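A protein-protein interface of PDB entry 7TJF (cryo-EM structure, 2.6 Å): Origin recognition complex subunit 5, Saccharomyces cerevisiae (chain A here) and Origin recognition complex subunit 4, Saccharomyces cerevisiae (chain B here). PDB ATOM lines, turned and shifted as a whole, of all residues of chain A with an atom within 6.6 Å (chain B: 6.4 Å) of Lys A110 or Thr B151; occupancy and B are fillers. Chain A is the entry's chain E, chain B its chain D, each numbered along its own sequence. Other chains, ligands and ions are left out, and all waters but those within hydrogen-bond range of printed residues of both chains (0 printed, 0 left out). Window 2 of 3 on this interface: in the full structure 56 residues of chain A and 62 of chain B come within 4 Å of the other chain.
The side-chain amide nitrogen (NE2) of Gln B155 lies within hydrogen-bond range of a ring nitrogen (ND1) of His A113 (3.1 Å).
The side-chain hydroxyl (OG1) of Thr B151 sits at hydrogen-bond distance from the backbone carbonyl oxygen (O) of Asn B147 (3.0 Å).
O of Lys A110 lies close to ND2 of Asn A114 (3.2 Å).
O of Gly B148 lies close to NE2 of Gln B152 (3.3 Å).
The backbone carbonyl oxygen (O) of Thr B151 sits close to the side-chain amide oxygen (OE1) of Gln B155 (3.2 Å).
Among the printed residues, pairs that only touch across the chains: Phe A106 with Gly B148 (3.5 Å), Phe A106 with Asn B147 (3.6 Å) and Lys A110 with Thr B151 (3.9 Å).
Printed residues of chain B within 4 Å of Phe A106: Asn B147 and Gly B148.
Of chain B, only Thr B151 comes within 4 Å of Lys A110.
Printed residues of chain B within 4 Å of His A113: Gln B155.
Of the printed residues of chain A, Asn B147 touches Phe A106 (3.6 Å).
Printed residues of chain A within 4 Å of Gly B148: Phe A106 (3.5 Å).
Thr B151 touches just one residue of chain A: Lys A110 (3.9 Å).
Printed residues of chain A within 4 Å of Gln B155: His A113 (3.1 Å).
The nearest residue of chain B that does not touch Lys A110 is Asn B147 (5.9 Å).
The nearest residue of chain A that does not touch Thr B151 is Phe A106 (4.3 Å).
Along chain B the printed residues that touch a printed residue of chain A span positions 147 to 155.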
ATOM      1  N   GLN A 101      15.392 -19.259 -17.299  1.00  0.00           N
ATOM      2  CA  GLN A 101      16.484 -19.236 -18.265  1.00  0.00           C
ATOM      3  C   GLN A 101      17.324 -20.505 -18.220  1.00  0.00           C
ATOM      4  O   GLN A 101      18.060 -20.778 -19.172  1.00  0.00           O
ATOM      5  CB  GLN A 101      17.382 -18.023 -18.027  1.00  0.00           C
ATOM      6  CG  GLN A 101      16.821 -16.716 -18.553  1.00  0.00           C
ATOM      7  CD  GLN A 101      17.902 -15.774 -19.036  1.00  0.00           C
ATOM      8  OE1 GLN A 101      18.339 -14.887 -18.306  1.00  0.00           O
ATOM      9  NE2 GLN A 101      18.344 -15.964 -20.275  1.00  0.00           N
ATOM     10  N   PRO A 105      21.694 -28.285 -18.495  1.00  0.00           N
ATOM     11  CA  PRO A 105      22.585 -28.431 -17.324  1.00  0.00           C
ATOM     12  C   PRO A 105      23.736 -27.436 -17.299  1.00  0.00           C
ATOM     13  O   PRO A 105      24.123 -26.966 -16.218  1.00  0.00           O
ATOM     14  CB  PRO A 105      23.088 -29.876 -17.448  1.00  0.00           C
ATOM     15  CG  PRO A 105      22.057 -30.574 -18.244  1.00  0.00           C
ATOM     16  CD  PRO A 105      21.462 -29.573 -19.176  1.00  0.00           C
ATOM     17  N   PHE A 106      24.283 -27.096 -18.473  1.00  0.00           N
ATOM     18  CA  PHE A 106      25.308 -26.060 -18.561  1.00  0.00           C
ATOM     19  C   PHE A 106      24.755 -24.705 -18.131  1.00  0.00           C
ATOM     20  O   PHE A 106      25.462 -23.908 -17.500  1.00  0.00           O
ATOM     21  CB  PHE A 106      25.869 -26.010 -19.990  1.00  0.00           C
ATOM     22  CG  PHE A 106      26.247 -24.629 -20.461  1.00  0.00           C
ATOM     23  CD1 PHE A 106      27.425 -24.023 -20.035  1.00  0.00           C
ATOM     24  CD2 PHE A 106      25.425 -23.940 -21.344  1.00  0.00           C
ATOM     25  CE1 PHE A 106      27.753 -22.752 -20.455  1.00  0.00           C
ATOM     26  CE2 PHE A 106      25.755 -22.672 -21.774  1.00  0.00           C
ATOM     27  CZ  PHE A 106      26.923 -22.079 -21.334  1.00  0.00           C
ATOM     28  N   LEU A 107      23.491 -24.429 -18.465  1.00  0.00           N
ATOM     29  CA  LEU A 107      22.848 -23.205 -18.006  1.00  0.00           C
ATOM     30  C   LEU A 107      22.659 -23.203 -16.494  1.00  0.00           C
ATOM     31  O   LEU A 107      22.752 -22.141 -15.869  1.00  0.00           O
ATOM     32  CB  LEU A 107      21.513 -23.014 -18.722  1.00  0.00           C
ATOM     33  CG  LEU A 107      21.639 -22.800 -20.232  1.00  0.00           C
ATOM     34  CD1 LEU A 107      20.281 -22.810 -20.906  1.00  0.00           C
ATOM     35  CD2 LEU A 107      22.388 -21.508 -20.533  1.00  0.00           C
ATOM     36  N   LEU A 108      22.423 -24.374 -15.892  1.00  0.00           N
ATOM     37  CA  LEU A 108      22.387 -24.461 -14.433  1.00  0.00           C
ATOM     38  C   LEU A 108      23.755 -24.174 -13.829  1.00  0.00           C
ATOM     39  O   LEU A 108      23.843 -23.493 -12.802  1.00  0.00           O
ATOM     40  CB  LEU A 108      21.887 -25.835 -13.981  1.00  0.00           C
ATOM     41  CG  LEU A 108      21.745 -25.966 -12.457  1.00  0.00           C
ATOM     42  CD1 LEU A 108      20.498 -25.248 -11.957  1.00  0.00           C
ATOM     43  CD2 LEU A 108      21.772 -27.408 -11.989  1.00  0.00           C
ATOM     44  N   VAL A 109      24.825 -24.664 -14.466  1.00  0.00           N
ATOM     45  CA  VAL A 109      26.186 -24.390 -13.992  1.00  0.00           C
ATOM     46  C   VAL A 109      26.486 -22.893 -14.051  1.00  0.00           C
ATOM     47  O   VAL A 109      26.982 -22.302 -13.081  1.00  0.00           O
ATOM     48  CB  VAL A 109      27.211 -25.202 -14.806  1.00  0.00           C
ATOM     49  CG1 VAL A 109      28.633 -24.819 -14.428  1.00  0.00           C
ATOM     50  CG2 VAL A 109      27.000 -26.689 -14.600  1.00  0.00           C
ATOM     51  N   LYS A 110      26.142 -22.258 -15.179  1.00  0.00           N
ATOM     52  CA  LYS A 110      26.368 -20.824 -15.354  1.00  0.00           C
ATOM     53  C   LYS A 110      25.549 -19.995 -14.369  1.00  0.00           C
ATOM     54  O   LYS A 110      26.067 -19.047 -13.762  1.00  0.00           O
ATOM     55  CB  LYS A 110      26.030 -20.421 -16.787  1.00  0.00           C
ATOM     56  CG  LYS A 110      26.389 -18.995 -17.143  1.00  0.00           C
ATOM     57  CD  LYS A 110      26.668 -18.867 -18.628  1.00  0.00           C
ATOM     58  CE  LYS A 110      25.408 -19.106 -19.445  1.00  0.00           C
ATOM     59  NZ  LYS A 110      24.603 -17.865 -19.617  1.00  0.00           N
ATOM     60  N   THR A 111      24.278 -20.359 -14.176  1.00  0.00           N
ATOM     61  CA  THR A 111      23.412 -19.625 -13.265  1.00  0.00           C
ATOM     62  C   THR A 111      23.852 -19.794 -11.816  1.00  0.00           C
ATOM     63  O   THR A 111      23.848 -18.824 -11.057  1.00  0.00           O
ATOM     64  CB  THR A 111      21.963 -20.077 -13.452  1.00  0.00           C
ATOM     65  OG1 THR A 111      21.641 -20.057 -14.848  1.00  0.00           O
ATOM     66  CG2 THR A 111      21.010 -19.162 -12.709  1.00  0.00           C
ATOM     67  N   LEU A 112      24.267 -21.004 -11.423  1.00  0.00           N
ATOM     68  CA  LEU A 112      24.750 -21.216 -10.061  1.00  0.00           C
ATOM     69  C   LEU A 112      26.061 -20.483  -9.813  1.00  0.00           C
ATOM     70  O   LEU A 112      26.283 -19.965  -8.714  1.00  0.00           O
ATOM     71  CB  LEU A 112      24.910 -22.709  -9.779  1.00  0.00           C
ATOM     72  CG  LEU A 112      23.640 -23.517  -9.510  1.00  0.00           C
ATOM     73  CD1 LEU A 112      23.986 -24.970  -9.247  1.00  0.00           C
ATOM     74  CD2 LEU A 112      22.848 -22.930  -8.356  1.00  0.00           C
ATOM     75  N   HIS A 113      26.934 -20.419 -10.825  1.00  0.00           N
ATOM     76  CA  HIS A 113      28.157 -19.629 -10.712  1.00  0.00           C
ATOM     77  C   HIS A 113      27.846 -18.146 -10.532  1.00  0.00           C
ATOM     78  O   HIS A 113      28.449 -17.475  -9.682  1.00  0.00           O
ATOM     79  CB  HIS A 113      29.025 -19.851 -11.951  1.00  0.00           C
ATOM     80  CG  HIS A 113      30.447 -19.417 -11.784  1.00  0.00           C
ATOM     81  ND1 HIS A 113      31.325 -19.316 -12.841  1.00  0.00           N
ATOM     82  CD2 HIS A 113      31.142 -19.058 -10.680  1.00  0.00           C
ATOM     83  CE1 HIS A 113      32.502 -18.912 -12.394  1.00  0.00           C
ATOM     84  NE2 HIS A 113      32.416 -18.748 -11.087  1.00  0.00           N
ATOM     85  N   ASN A 114      26.880 -17.629 -11.300  1.00  0.00           N
ATOM     86  CA  ASN A 114      26.490 -16.227 -11.179  1.00  0.00           C
ATOM     87  C   ASN A 114      25.794 -15.937  -9.854  1.00  0.00           C
ATOM     88  O   ASN A 114      25.889 -14.818  -9.338  1.00  0.00           O
ATOM     89  CB  ASN A 114      25.582 -15.839 -12.344  1.00  0.00           C
ATOM     90  CG  ASN A 114      26.296 -15.880 -13.674  1.00  0.00           C
ATOM     91  OD1 ASN A 114      27.520 -15.797 -13.735  1.00  0.00           O
ATOM     92  ND2 ASN A 114      25.531 -16.012 -14.750  1.00  0.00           N
ATOM     93  N   ILE A 115      25.073 -16.916  -9.307  1.00  0.00           N
ATOM     94  CA  ILE A 115      24.461 -16.760  -7.992  1.00  0.00           C
ATOM     95  C   ILE A 115      25.531 -16.754  -6.905  1.00  0.00           C
ATOM     96  O   ILE A 115      25.489 -15.941  -5.977  1.00  0.00           O
ATOM     97  CB  ILE A 115      23.414 -17.873  -7.773  1.00  0.00           C
ATOM     98  CG1 ILE A 115      22.168 -17.619  -8.618  1.00  0.00           C
ATOM     99  CG2 ILE A 115      22.984 -17.970  -6.320  1.00  0.00           C
ATOM    100  CD1 ILE A 115      21.328 -18.867  -8.817  1.00  0.00           C
ATOM    101  N   LEU A 156      31.905 -26.187 -11.000  1.00  0.00           N
ATOM    102  CA  LEU A 156      31.760 -25.045 -10.118  1.00  0.00           C
ATOM    103  C   LEU A 156      33.098 -24.721  -9.457  1.00  0.00           C
ATOM    104  O   LEU A 156      33.942 -25.611  -9.310  1.00  0.00           O
ATOM    105  CB  LEU A 156      30.687 -25.339  -9.063  1.00  0.00           C
ATOM    106  CG  LEU A 156      29.284 -25.295  -9.673  1.00  0.00           C
ATOM    107  CD1 LEU A 156      28.234 -25.685  -8.665  1.00  0.00           C
ATOM    108  CD2 LEU A 156      28.990 -23.911 -10.242  1.00  0.00           C
ATOM    109  N   ILE B 133      40.035 -24.220 -19.352  1.00  0.00           N
ATOM    110  CA  ILE B 133      38.669 -24.464 -19.805  1.00  0.00           C
ATOM    111  C   ILE B 133      38.359 -25.929 -19.534  1.00  0.00           C
ATOM    112  O   ILE B 133      39.041 -26.816 -20.060  1.00  0.00           O
ATOM    113  CB  ILE B 133      38.492 -24.146 -21.300  1.00  0.00           C
ATOM    114  CG1 ILE B 133      39.239 -22.864 -21.686  1.00  0.00           C
ATOM    115  CG2 ILE B 133      37.014 -24.075 -21.668  1.00  0.00           C
ATOM    116  CD1 ILE B 133      38.618 -21.597 -21.161  1.00  0.00           C
ATOM    117  N   ILE B 146      30.237 -25.325 -27.006  1.00  0.00           N
ATOM    118  CA  ILE B 146      30.737 -24.091 -27.608  1.00  0.00           C
ATOM    119  C   ILE B 146      30.448 -22.896 -26.705  1.00  0.00           C
ATOM    120  O   ILE B 146      31.322 -22.048 -26.464  1.00  0.00           O
ATOM    121  CB  ILE B 146      30.120 -23.917 -29.009  1.00  0.00           C
ATOM    122  CG1 ILE B 146      30.577 -25.048 -29.930  1.00  0.00           C
ATOM    123  CG2 ILE B 146      30.474 -22.572 -29.613  1.00  0.00           C
ATOM    124  CD1 ILE B 146      29.606 -25.354 -31.034  1.00  0.00           C
ATOM    125  N   ASN B 147      29.225 -22.832 -26.166  1.00  0.00           N
ATOM    126  CA  ASN B 147      28.854 -21.780 -25.225  1.00  0.00           C
ATOM    127  C   ASN B 147      29.662 -21.874 -23.939  1.00  0.00           C
ATOM    128  O   ASN B 147      30.062 -20.848 -23.376  1.00  0.00           O
ATOM    129  CB  ASN B 147      27.358 -21.859 -24.925  1.00  0.00           C
ATOM    130  CG  ASN B 147      26.538 -20.948 -25.811  1.00  0.00           C
ATOM    131  OD1 ASN B 147      26.840 -20.769 -26.988  1.00  0.00           O
ATOM    132  ND2 ASN B 147      25.491 -20.364 -25.246  1.00  0.00           N
ATOM    133  N   GLY B 148      29.919 -23.098 -23.467  1.00  0.00           N
ATOM    134  CA  GLY B 148      30.730 -23.277 -22.274  1.00  0.00           C
ATOM    135  C   GLY B 148      32.171 -22.852 -22.468  1.00  0.00           C
ATOM    136  O   GLY B 148      32.760 -22.223 -21.584  1.00  0.00           O
ATOM    137  N   ILE B 149      32.743 -23.171 -23.633  1.00  0.00           N
ATOM    138  CA  ILE B 149      34.102 -22.754 -23.968  1.00  0.00           C
ATOM    139  C   ILE B 149      34.193 -21.234 -24.027  1.00  0.00           C
ATOM    140  O   ILE B 149      35.106 -20.634 -23.451  1.00  0.00           O
ATOM    141  CB  ILE B 149      34.549 -23.407 -25.290  1.00  0.00           C
ATOM    142  CG1 ILE B 149      34.911 -24.876 -25.069  1.00  0.00           C
ATOM    143  CG2 ILE B 149      35.733 -22.675 -25.909  1.00  0.00           C
ATOM    144  CD1 ILE B 149      34.940 -25.681 -26.338  1.00  0.00           C
ATOM    145  N   ALA B 150      33.216 -20.590 -24.682  1.00  0.00           N
ATOM    146  CA  ALA B 150      33.235 -19.132 -24.807  1.00  0.00           C
ATOM    147  C   ALA B 150      33.049 -18.439 -23.459  1.00  0.00           C
ATOM    148  O   ALA B 150      33.750 -17.459 -23.158  1.00  0.00           O
ATOM    149  CB  ALA B 150      32.162 -18.681 -25.794  1.00  0.00           C
ATOM    150  N   THR B 151      32.132 -18.947 -22.630  1.00  0.00           N
ATOM    151  CA  THR B 151      31.899 -18.371 -21.308  1.00  0.00           C
ATOM    152  C   THR B 151      33.124 -18.527 -20.414  1.00  0.00           C
ATOM    153  O   THR B 151      33.570 -17.561 -19.781  1.00  0.00           O
ATOM    154  CB  THR B 151      30.669 -19.024 -20.672  1.00  0.00           C
ATOM    155  OG1 THR B 151      29.501 -18.671 -21.422  1.00  0.00           O
ATOM    156  CG2 THR B 151      30.484 -18.561 -19.237  1.00  0.00           C
ATOM    157  N   GLN B 152      33.713 -19.727 -20.389  1.00  0.00           N
ATOM    158  CA  GLN B 152      34.900 -19.953 -19.576  1.00  0.00           C
ATOM    159  C   GLN B 152      36.093 -19.152 -20.077  1.00  0.00           C
ATOM    160  O   GLN B 152      36.894 -18.682 -19.265  1.00  0.00           O
ATOM    161  CB  GLN B 152      35.233 -21.439 -19.541  1.00  0.00           C
ATOM    162  CG  GLN B 152      34.338 -22.243 -18.628  1.00  0.00           C
ATOM    163  CD  GLN B 152      34.676 -23.711 -18.652  1.00  0.00           C
ATOM    164  OE1 GLN B 152      35.606 -24.153 -17.981  1.00  0.00           O
ATOM    165  NE2 GLN B 152      33.931 -24.478 -19.437  1.00  0.00           N
ATOM    166  N   LEU B 153      36.200 -18.949 -21.396  1.00  0.00           N
ATOM    167  CA  LEU B 153      37.251 -18.103 -21.952  1.00  0.00           C
ATOM    168  C   LEU B 153      37.102 -16.661 -21.486  1.00  0.00           C
ATOM    169  O   LEU B 153      38.084 -16.027 -21.079  1.00  0.00           O
ATOM    170  CB  LEU B 153      37.225 -18.174 -23.479  1.00  0.00           C
ATOM    171  CG  LEU B 153      38.037 -19.254 -24.194  1.00  0.00           C
ATOM    172  CD1 LEU B 153      37.586 -19.363 -25.638  1.00  0.00           C
ATOM    173  CD2 LEU B 153      39.521 -18.966 -24.119  1.00  0.00           C
ATOM    174  N   GLU B 154      35.871 -16.136 -21.508  1.00  0.00           N
ATOM    175  CA  GLU B 154      35.689 -14.736 -21.135  1.00  0.00           C
ATOM    176  C   GLU B 154      35.870 -14.509 -19.634  1.00  0.00           C
ATOM    177  O   GLU B 154      36.331 -13.435 -19.238  1.00  0.00           O
ATOM    178  CB  GLU B 154      34.351 -14.206 -21.712  1.00  0.00           C
ATOM    179  CG  GLU B 154      32.946 -14.737 -21.274  1.00  0.00           C
ATOM    180  CD  GLU B 154      32.537 -14.630 -19.802  1.00  0.00           C
ATOM    181  OE1 GLU B 154      33.064 -13.792 -19.044  1.00  0.00           O
ATOM    182  OE2 GLU B 154      31.549 -15.301 -19.438  1.00  0.00           O
ATOM    183  N   GLN B 155      35.531 -15.484 -18.778  1.00  0.00           N
ATOM    184  CA  GLN B 155      35.877 -15.279 -17.365  1.00  0.00           C
ATOM    185  C   GLN B 155      37.355 -15.517 -17.067  1.00  0.00           C
ATOM    186  O   GLN B 155      37.932 -14.805 -16.230  1.00  0.00           O
ATOM    187  CB  GLN B 155      35.021 -16.136 -16.426  1.00  0.00           C
ATOM    188  CG  GLN B 155      33.601 -16.362 -16.862  1.00  0.00           C
ATOM    189  CD  GLN B 155      32.997 -17.612 -16.267  1.00  0.00           C
ATOM    190  OE1 GLN B 155      33.177 -18.713 -16.787  1.00  0.00           O
ATOM    191  NE2 GLN B 155      32.267 -17.449 -15.174  1.00  0.00           N
ATOM    192  N   GLN B 156      37.998 -16.481 -17.734  1.00  0.00           N
ATOM    193  CA  GLN B 156      39.395 -16.761 -17.424  1.00  0.00           C
ATOM    194  C   GLN B 156      40.318 -15.678 -17.968  1.00  0.00           C
ATOM    195  O   GLN B 156      41.400 -15.458 -17.416  1.00  0.00           O
ATOM    196  CB  GLN B 156      39.793 -18.131 -17.969  1.00  0.00           C
ATOM    197  CG  GLN B 156      39.276 -19.303 -17.144  1.00  0.00           C
ATOM    198  CD  GLN B 156      40.267 -19.799 -16.122  1.00  0.00           C
ATOM    199  OE1 GLN B 156      41.476 -19.711 -16.317  1.00  0.00           O
ATOM    200  NE2 GLN B 156      39.758 -20.342 -15.027  1.00  0.00           N
ATOM    201  N   ILE B 175      33.274 -12.679 -26.717  1.00  0.00           N
ATOM    202  CA  ILE B 175      33.294 -13.943 -27.445  1.00  0.00           C
ATOM    203  C   ILE B 175      31.947 -14.650 -27.336  1.00  0.00           C
ATOM    204  O   ILE B 175      31.453 -15.230 -28.311  1.00  0.00           O
ATOM    205  CB  ILE B 175      34.439 -14.826 -26.916  1.00  0.00           C
ATOM    206  CG1 ILE B 175      35.738 -14.028 -26.872  1.00  0.00           C
ATOM    207  CG2 ILE B 175      34.623 -16.055 -27.789  1.00  0.00           C
ATOM    208  CD1 ILE B 175      36.602 -14.357 -25.684  1.00  0.00           C
ATOM    209  N   SER B 176      31.328 -14.601 -26.157  1.00  0.00           N
ATOM    210  CA  SER B 176      30.154 -15.415 -25.869  1.00  0.00           C
ATOM    211  C   SER B 176      28.851 -14.813 -26.379  1.00  0.00           C
ATOM    212  O   SER B 176      27.824 -15.500 -26.354  1.00  0.00           O
ATOM    213  CB  SER B 176      30.055 -15.662 -24.362  1.00  0.00           C
ATOM    214  OG  SER B 176      29.114 -14.793 -23.761  1.00  0.00           O
